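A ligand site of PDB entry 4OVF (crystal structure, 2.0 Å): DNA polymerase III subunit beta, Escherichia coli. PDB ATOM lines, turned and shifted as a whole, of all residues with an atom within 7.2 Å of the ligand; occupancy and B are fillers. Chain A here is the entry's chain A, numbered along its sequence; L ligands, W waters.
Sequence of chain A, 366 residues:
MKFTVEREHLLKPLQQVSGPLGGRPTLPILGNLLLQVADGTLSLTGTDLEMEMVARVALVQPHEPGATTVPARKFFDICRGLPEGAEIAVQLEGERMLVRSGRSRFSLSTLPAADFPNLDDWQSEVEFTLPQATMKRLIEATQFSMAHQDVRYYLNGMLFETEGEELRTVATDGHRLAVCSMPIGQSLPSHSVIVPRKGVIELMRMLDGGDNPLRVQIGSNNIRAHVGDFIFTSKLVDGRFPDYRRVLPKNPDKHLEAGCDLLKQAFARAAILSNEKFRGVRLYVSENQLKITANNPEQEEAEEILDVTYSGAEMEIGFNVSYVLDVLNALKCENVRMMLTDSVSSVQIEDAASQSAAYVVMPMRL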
ATOM      1  N   ASP A 150       1.924 -10.790  31.050  1.00  0.00           N
ATOM      2  CA  ASP A 150       0.481 -10.619  31.237  1.00  0.00           C
ATOM      3  C   ASP A 150      -0.116 -11.941  31.723  1.00  0.00           C
ATOM      4  O   ASP A 150       0.328 -13.007  31.306  1.00  0.00           O
ATOM      5  CB  ASP A 150      -0.162 -10.215  29.900  1.00  0.00           C
ATOM      6  CG  ASP A 150      -1.594  -9.743  30.049  1.00  0.00           C
ATOM      7  OD1 ASP A 150      -2.476 -10.556  30.392  1.00  0.00           O
ATOM      8  OD2 ASP A 150      -1.853  -8.548  29.800  1.00  0.00           O
ATOM      9  N   ARG A 152      -2.855 -13.148  30.867  1.00  0.00           N
ATOM     10  CA  ARG A 152      -3.294 -13.833  29.656  1.00  0.00           C
ATOM     11  C   ARG A 152      -2.041 -14.356  28.970  1.00  0.00           C
ATOM     12  O   ARG A 152      -1.435 -13.673  28.149  1.00  0.00           O
ATOM     13  CB  ARG A 152      -4.098 -12.909  28.739  1.00  0.00           C
ATOM     14  CG  ARG A 152      -5.393 -12.398  29.356  1.00  0.00           C
ATOM     15  CD  ARG A 152      -5.273 -10.921  29.679  1.00  0.00           C
ATOM     16  NE  ARG A 152      -6.003 -10.114  28.717  1.00  0.00           N
ATOM     17  CZ  ARG A 152      -5.727  -8.854  28.395  1.00  0.00           C
ATOM     18  NH1 ARG A 152      -4.682  -8.217  28.917  1.00  0.00           N
ATOM     19  NH2 ARG A 152      -6.489  -8.238  27.508  1.00  0.00           N
ATOM     20  N   TYR A 154      -1.369 -16.396  26.727  1.00  0.00           N
ATOM     21  CA  TYR A 154      -1.359 -16.490  25.271  1.00  0.00           C
ATOM     22  C   TYR A 154      -0.895 -15.192  24.580  1.00  0.00           C
ATOM     23  O   TYR A 154      -0.601 -15.197  23.399  1.00  0.00           O
ATOM     24  CB  TYR A 154      -2.725 -16.949  24.747  1.00  0.00           C
ATOM     25  CG  TYR A 154      -3.917 -16.153  25.259  1.00  0.00           C
ATOM     26  CD1 TYR A 154      -4.313 -14.972  24.625  1.00  0.00           C
ATOM     27  CD2 TYR A 154      -4.644 -16.590  26.367  1.00  0.00           C
ATOM     28  CE1 TYR A 154      -5.398 -14.245  25.093  1.00  0.00           C
ATOM     29  CE2 TYR A 154      -5.723 -15.877  26.843  1.00  0.00           C
ATOM     30  CZ  TYR A 154      -6.100 -14.708  26.199  1.00  0.00           C
ATOM     31  OH  TYR A 154      -7.174 -14.009  26.683  1.00  0.00           O
ATOM     32  N   LEU A 155      -0.841 -14.097  25.334  1.00  0.00           N
ATOM     33  CA  LEU A 155      -0.397 -12.796  24.801  1.00  0.00           C
ATOM     34  C   LEU A 155       1.099 -12.546  24.987  1.00  0.00           C
ATOM     35  O   LEU A 155       1.659 -11.651  24.356  1.00  0.00           O
ATOM     36  CB  LEU A 155      -1.202 -11.634  25.417  1.00  0.00           C
ATOM     37  CG  LEU A 155      -2.710 -11.538  25.199  1.00  0.00           C
ATOM     38  CD1 LEU A 155      -3.237 -10.235  25.813  1.00  0.00           C
ATOM     39  CD2 LEU A 155      -3.119 -11.638  23.735  1.00  0.00           C
ATOM     40  N   ALA A 171       1.009  -9.851  17.054  1.00  0.00           N
ATOM     41  CA  ALA A 171       1.376  -9.599  18.442  1.00  0.00           C
ATOM     42  C   ALA A 171       0.515  -8.495  19.005  1.00  0.00           C
ATOM     43  O   ALA A 171       0.318  -7.446  18.365  1.00  0.00           O
ATOM     44  CB  ALA A 171       2.845  -9.231  18.548  1.00  0.00           C
ATOM     45  N   THR A 172       0.019  -8.730  20.212  1.00  0.00           N
ATOM     46  CA  THR A 172      -0.833  -7.779  20.905  1.00  0.00           C
ATOM     47  C   THR A 172      -0.693  -7.958  22.419  1.00  0.00           C
ATOM     48  O   THR A 172      -0.426  -9.062  22.901  1.00  0.00           O
ATOM     49  CB  THR A 172      -2.314  -7.887  20.452  1.00  0.00           C
ATOM     50  OG1 THR A 172      -3.101  -6.867  21.064  1.00  0.00           O
ATOM     51  CG2 THR A 172      -2.902  -9.268  20.762  1.00  0.00           C
ATOM     52  N   ASP A 173      -0.853  -6.858  23.149  1.00  0.00           N
ATOM     53  CA  ASP A 173      -0.867  -6.887  24.622  1.00  0.00           C
ATOM     54  C   ASP A 173      -2.218  -6.468  25.196  1.00  0.00           C
ATOM     55  O   ASP A 173      -2.318  -6.147  26.382  1.00  0.00           O
ATOM     56  CB  ASP A 173       0.267  -6.018  25.203  1.00  0.00           C
ATOM     57  CG  ASP A 173       0.186  -4.556  24.768  1.00  0.00           C
ATOM     58  OD1 ASP A 173      -0.847  -4.117  24.230  1.00  0.00           O
ATOM     59  OD2 ASP A 173       1.179  -3.826  24.980  1.00  0.00           O
ATOM     60  N   GLY A 174      -3.247  -6.454  24.363  1.00  0.00           N
ATOM     61  CA  GLY A 174      -4.571  -5.973  24.769  1.00  0.00           C
ATOM     62  C   GLY A 174      -4.817  -4.485  24.567  1.00  0.00           C
ATOM     63  O   GLY A 174      -5.966  -4.053  24.554  1.00  0.00           O
ATOM     64  N   HIS A 175      -3.746  -3.702  24.396  1.00  0.00           N
ATOM     65  CA  HIS A 175      -3.871  -2.248  24.226  1.00  0.00           C
ATOM     66  C   HIS A 175      -3.481  -1.789  22.830  1.00  0.00           C
ATOM     67  O   HIS A 175      -3.974  -0.765  22.328  1.00  0.00           O
ATOM     68  CB  HIS A 175      -3.014  -1.503  25.256  1.00  0.00           C
ATOM     69  CG  HIS A 175      -3.209  -1.968  26.661  1.00  0.00           C
ATOM     70  ND1 HIS A 175      -4.351  -1.691  27.380  1.00  0.00           N
ATOM     71  CD2 HIS A 175      -2.413  -2.716  27.476  1.00  0.00           C
ATOM     72  CE1 HIS A 175      -4.253  -2.238  28.581  1.00  0.00           C
ATOM     73  NE2 HIS A 175      -3.081  -2.858  28.663  1.00  0.00           N
ATOM     74  N   ARG A 176      -2.570  -2.530  22.214  1.00  0.00           N
ATOM     75  CA  ARG A 176      -2.160  -2.266  20.842  1.00  0.00           C
ATOM     76  C   ARG A 176      -1.849  -3.577  20.145  1.00  0.00           C
ATOM     77  O   ARG A 176      -1.570  -4.581  20.799  1.00  0.00           O
ATOM     78  CB  ARG A 176      -0.968  -1.296  20.779  1.00  0.00           C
ATOM     79  CG  ARG A 176       0.081  -1.444  21.870  1.00  0.00           C
ATOM     80  CD  ARG A 176       1.113  -2.521  21.544  1.00  0.00           C
ATOM     81  NE  ARG A 176       2.095  -2.627  22.608  1.00  0.00           N
ATOM     82  CZ  ARG A 176       3.173  -1.838  22.731  1.00  0.00           C
ATOM     83  NH1 ARG A 176       3.412  -0.880  21.837  1.00  0.00           N
ATOM     84  NH2 ARG A 176       3.997  -2.017  23.751  1.00  0.00           N
ATOM     85  N   LEU A 177      -1.900  -3.572  18.809  1.00  0.00           N
ATOM     86  CA  LEU A 177      -1.669  -4.771  18.016  1.00  0.00           C
ATOM     87  C   LEU A 177      -0.780  -4.465  16.828  1.00  0.00           C
ATOM     88  O   LEU A 177      -0.845  -3.378  16.256  1.00  0.00           O
ATOM     89  CB  LEU A 177      -3.016  -5.359  17.545  1.00  0.00           C
ATOM     90  CG  LEU A 177      -3.045  -6.559  16.584  1.00  0.00           C
ATOM     91  CD1 LEU A 177      -4.104  -7.565  16.995  1.00  0.00           C
ATOM     92  CD2 LEU A 177      -3.219  -6.128  15.135  1.00  0.00           C
ATOM     93  N   ALA A 178       0.032  -5.444  16.461  1.00  0.00           N
ATOM     94  CA  ALA A 178       0.803  -5.425  15.233  1.00  0.00           C
ATOM     95  C   ALA A 178       0.532  -6.723  14.469  1.00  0.00           C
ATOM     96  O   ALA A 178       0.487  -7.809  15.065  1.00  0.00           O
ATOM     97  CB  ALA A 178       2.290  -5.308  15.561  1.00  0.00           C
ATOM     98  N   ARG A 240      -6.453 -19.334  23.291  1.00  0.00           N
ATOM     99  CA  ARG A 240      -7.102 -18.790  22.112  1.00  0.00           C
ATOM    100  C   ARG A 240      -6.647 -17.350  21.858  1.00  0.00           C
ATOM    101  O   ARG A 240      -7.124 -16.408  22.499  1.00  0.00           O
ATOM    102  CB  ARG A 240      -8.625 -18.847  22.254  1.00  0.00           C
ATOM    103  CG  ARG A 240      -9.231 -20.194  21.848  1.00  0.00           C
ATOM    104  CD  ARG A 240     -10.197 -20.757  22.886  1.00  0.00           C
ATOM    105  NE  ARG A 240     -10.920 -19.738  23.655  1.00  0.00           N
ATOM    106  CZ  ARG A 240     -11.975 -19.059  23.213  1.00  0.00           C
ATOM    107  NH1 ARG A 240     -12.440 -19.274  21.991  1.00  0.00           N
ATOM    108  NH2 ARG A 240     -12.562 -18.155  23.996  1.00  0.00           N
ATOM    109  N   PHE A 241      -5.713 -17.204  20.927  1.00  0.00           N
ATOM    110  CA  PHE A 241      -5.210 -15.896  20.529  1.00  0.00           C
ATOM    111  C   PHE A 241      -6.354 -15.079  19.920  1.00  0.00           C
ATOM    112  O   PHE A 241      -7.205 -15.626  19.219  1.00  0.00           O
ATOM    113  CB  PHE A 241      -4.066 -16.047  19.535  1.00  0.00           C
ATOM    114  CG  PHE A 241      -3.112 -14.891  19.528  1.00  0.00           C
ATOM    115  CD1 PHE A 241      -2.091 -14.812  20.472  1.00  0.00           C
ATOM    116  CD2 PHE A 241      -3.228 -13.882  18.585  1.00  0.00           C
ATOM    117  CE1 PHE A 241      -1.215 -13.744  20.483  1.00  0.00           C
ATOM    118  CE2 PHE A 241      -2.345 -12.799  18.580  1.00  0.00           C
ATOM    119  CZ  PHE A 241      -1.338 -12.730  19.529  1.00  0.00           C
ATOM    120  N   PRO A 242      -6.385 -13.767  20.209  1.00  0.00           N
ATOM    121  CA  PRO A 242      -7.385 -12.895  19.579  1.00  0.00           C
ATOM    122  C   PRO A 242      -7.271 -12.887  18.052  1.00  0.00           C
ATOM    123  O   PRO A 242      -6.201 -13.111  17.501  1.00  0.00           O
ATOM    124  CB  PRO A 242      -7.041 -11.509  20.141  1.00  0.00           C
ATOM    125  CG  PRO A 242      -5.661 -11.634  20.704  1.00  0.00           C
ATOM    126  CD  PRO A 242      -5.612 -13.033  21.223  1.00  0.00           C
ATOM    127  N   ASP A 243      -8.397 -12.616  17.396  1.00  0.00           N
ATOM    128  CA  ASP A 243      -8.478 -12.541  15.933  1.00  0.00           C
ATOM    129  C   ASP A 243      -8.170 -11.118  15.495  1.00  0.00           C
ATOM    130  O   ASP A 243      -8.941 -10.197  15.792  1.00  0.00           O
ATOM    131  CB  ASP A 243      -9.882 -12.971  15.471  1.00  0.00           C
ATOM    132  CG  ASP A 243     -10.102 -12.805  13.975  1.00  0.00           C
ATOM    133  OD1 ASP A 243      -9.144 -12.559  13.208  1.00  0.00           O
ATOM    134  OD2 ASP A 243     -11.266 -12.933  13.536  1.00  0.00           O
ATOM    135  N   VAL A 247      -9.827  -6.683  15.565  1.00  0.00           N
ATOM    136  CA  VAL A 247      -9.105  -5.549  16.124  1.00  0.00           C
ATOM    137  C   VAL A 247      -8.935  -4.448  15.070  1.00  0.00           C
ATOM    138  O   VAL A 247      -9.067  -3.267  15.390  1.00  0.00           O
ATOM    139  CB  VAL A 247      -7.741  -5.977  16.701  1.00  0.00           C
ATOM    140  CG1 VAL A 247      -7.026  -4.786  17.317  1.00  0.00           C
ATOM    141  CG2 VAL A 247      -7.909  -7.091  17.730  1.00  0.00           C
ATOM    142  N   LEU A 248      -8.623  -4.845  13.833  1.00  0.00           N
ATOM    143  CA  LEU A 248      -8.598  -3.902  12.727  1.00  0.00           C
ATOM    144  C   LEU A 248      -9.954  -3.220  12.592  1.00  0.00           C
ATOM    145  O   LEU A 248     -10.988  -3.896  12.556  1.00  0.00           O
ATOM    146  CB  LEU A 248      -8.258  -4.586  11.403  1.00  0.00           C
ATOM    147  CG  LEU A 248      -6.858  -5.159  11.130  1.00  0.00           C
ATOM    148  CD1 LEU A 248      -6.849  -5.818   9.757  1.00  0.00           C
ATOM    149  CD2 LEU A 248      -5.786  -4.089  11.216  1.00  0.00           C
ATOM    150  N   SER A 346     -10.425   2.818  17.658  1.00  0.00           N
ATOM    151  CA  SER A 346      -9.008   2.586  17.414  1.00  0.00           C
ATOM    152  C   SER A 346      -8.536   3.248  16.131  1.00  0.00           C
ATOM    153  O   SER A 346      -9.339   3.545  15.258  1.00  0.00           O
ATOM    154  CB  SER A 346      -8.739   1.085  17.329  1.00  0.00           C
ATOM    155  OG  SER A 346      -8.690   0.504  18.625  1.00  0.00           O
ATOM    156  N   TYR A 359      -0.879  -1.723  12.091  1.00  0.00           N
ATOM    157  CA  TYR A 359      -0.770  -1.469  13.518  1.00  0.00           C
ATOM    158  C   TYR A 359      -2.066  -0.859  14.003  1.00  0.00           C
ATOM    159  O   TYR A 359      -2.644  -0.023  13.315  1.00  0.00           O
ATOM    160  CB  TYR A 359       0.428  -0.556  13.775  1.00  0.00           C
ATOM    161  CG  TYR A 359       1.702  -1.187  13.268  1.00  0.00           C
ATOM    162  CD1 TYR A 359       2.440  -2.040  14.080  1.00  0.00           C
ATOM    163  CD2 TYR A 359       2.140  -0.979  11.951  1.00  0.00           C
ATOM    164  CE1 TYR A 359       3.598  -2.643  13.614  1.00  0.00           C
ATOM    165  CE2 TYR A 359       3.297  -1.581  11.486  1.00  0.00           C
ATOM    166  CZ  TYR A 359       4.022  -2.422  12.330  1.00  0.00           C
ATOM    167  OH  TYR A 359       5.160  -3.039  11.887  1.00  0.00           O
ATOM    168  N   VAL A 360      -2.525  -1.311  15.167  1.00  0.00           N
ATOM    169  CA  VAL A 360      -3.764  -0.784  15.739  1.00  0.00           C
ATOM    170  C   VAL A 360      -3.512  -0.305  17.153  1.00  0.00           C
ATOM    171  O   VAL A 360      -2.893  -1.008  17.965  1.00  0.00           O
ATOM    172  CB  VAL A 360      -4.917  -1.818  15.686  1.00  0.00           C
ATOM    173  CG1 VAL A 360      -6.162  -1.284  16.398  1.00  0.00           C
ATOM    174  CG2 VAL A 360      -5.251  -2.179  14.253  1.00  0.00           C
ATOM    175  N   VAL A 361      -3.962   0.917  17.430  1.00  0.00           N
ATOM    176  CA  VAL A 361      -3.836   1.500  18.765  1.00  0.00           C
ATOM    177  C   VAL A 361      -5.187   2.014  19.249  1.00  0.00           C
ATOM    178  O   VAL A 361      -5.885   2.729  18.537  1.00  0.00           O
ATOM    179  CB  VAL A 361      -2.759   2.616  18.778  1.00  0.00           C
ATOM    180  CG1 VAL A 361      -2.521   3.128  20.197  1.00  0.00           C
ATOM    181  CG2 VAL A 361      -1.440   2.108  18.201  1.00  0.00           C
ATOM    182  N   MET A 362      -5.570   1.607  20.458  1.00  0.00           N
ATOM    183  CA  MET A 362      -6.826   2.024  21.079  1.00  0.00           C
ATOM    184  C   MET A 362      -6.766   3.469  21.560  1.00  0.00           C
ATOM    185  O   MET A 362      -5.698   3.951  21.925  1.00  0.00           O
ATOM    186  CB  MET A 362      -7.174   1.113  22.269  1.00  0.00           C
ATOM    187  CG  MET A 362      -7.632  -0.271  21.860  1.00  0.00           C
ATOM    188  SD  MET A 362      -9.279  -0.276  21.101  1.00  0.00           S
ATOM    189  CE  MET A 362     -10.304  -0.498  22.557  1.00  0.00           C
HETATM  190 CL1  LIG L   1      -5.314  -3.286  19.821  1.00  0.00          CL
HETATM  191  C1  LIG L   1      -6.432  -4.153  20.923  1.00  0.00           C
HETATM  192  C2  LIG L   1      -6.222  -5.481  21.303  1.00  0.00           C
HETATM  193  C3  LIG L   1      -7.149  -6.074  22.160  1.00  0.00           C
HETATM  194  C4  LIG L   1      -7.537  -3.450  21.411  1.00  0.00           C
HETATM  195  C5  LIG L   1      -8.446  -4.058  22.268  1.00  0.00           C
HETATM  196  C6  LIG L   1      -8.254  -5.371  22.647  1.00  0.00           C
HETATM  197  N1  LIG L   1      -8.956  -6.193  23.455  1.00  0.00           N
HETATM  198  C7  LIG L   1      -8.344  -7.387  23.509  1.00  0.00           C
HETATM  199  C8  LIG L   1      -7.210  -7.345  22.709  1.00  0.00           C
HETATM  200  C9  LIG L   1      -6.268  -8.505  22.518  1.00  0.00           C
HETATM  201  C10 LIG L   1      -6.456  -9.446  23.710  1.00  0.00           C
HETATM  202  C11 LIG L   1      -8.792  -8.592  24.296  1.00  0.00           C
HETATM  203  C12 LIG L   1      -7.913  -9.814  23.973  1.00  0.00           C
HETATM  204  C13 LIG L   1      -7.956 -10.797  25.116  1.00  0.00           C
HETATM  205  O1  LIG L   1      -8.194 -10.396  26.363  1.00  0.00           O
HETATM  206  O2  LIG L   1      -7.773 -11.976  24.919  1.00  0.00           O
HETATM  207  O   HOH W   1     -10.372  -8.892  27.193  1.00  0.00           O
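The guanidinium group of Arg 152 is in salt-bridge range of an oxygen (O1) of the ligand, at 3.0 Å. The side-chain hydroxyl (OH) of Tyr 154 lies within hydrogen-bond range of an oxygen (O2) of the ligand, 2.8 Å away.
NE of Arg 176 is in salt-bridge range of OD2 of Asp 173, at 2.8 Å. O of Arg 176 lies within hydrogen-bond range of OG1 of Thr 172 (2.8 Å). The backbone NH (N) of His 175 is in hydrogen-bond range of the side-chain carboxylate (OD1) of Asp 173 (2.9 Å). NH1 of Arg 152 lies within salt-bridge range of OD2 of Asp 150 (3.0 Å). The backbone NH of Met 362 lies within hydrogen-bond range of the backbone carbonyl oxygen of His 175 (3.4 Å). The side-chain hydroxyl of Ser 346 is in hydrogen-bond range of the side-chain sulfur of Met 362 (2.7 Å). The backbone NH (N) of Leu 177 sits at hydrogen-bond distance from the backbone carbonyl oxygen (O) of Val 360. The backbone NH of Gly 174 lies within hydrogen-bond range of the side-chain hydroxyl of Thr 172 (3.3 Å).
Merely in contact with the ligand: Met 362, Gly 174, Val 247, Thr 172, Arg 176, Leu 177, Pro 242, His 175, Val 360 and Leu 155. Hydrophobic or aromatic side chains that line the ligand: Tyr 154, Leu 155, Leu 177, Pro 242, Val 247 and Met 362. 12 residues have an atom within 4 Å of the ligand: Arg 152, Tyr 154, Leu 155, Thr 172, Gly 174, His 175, Arg 176, Leu 177, Pro 242, Val 247, Val 360 and Met 362.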
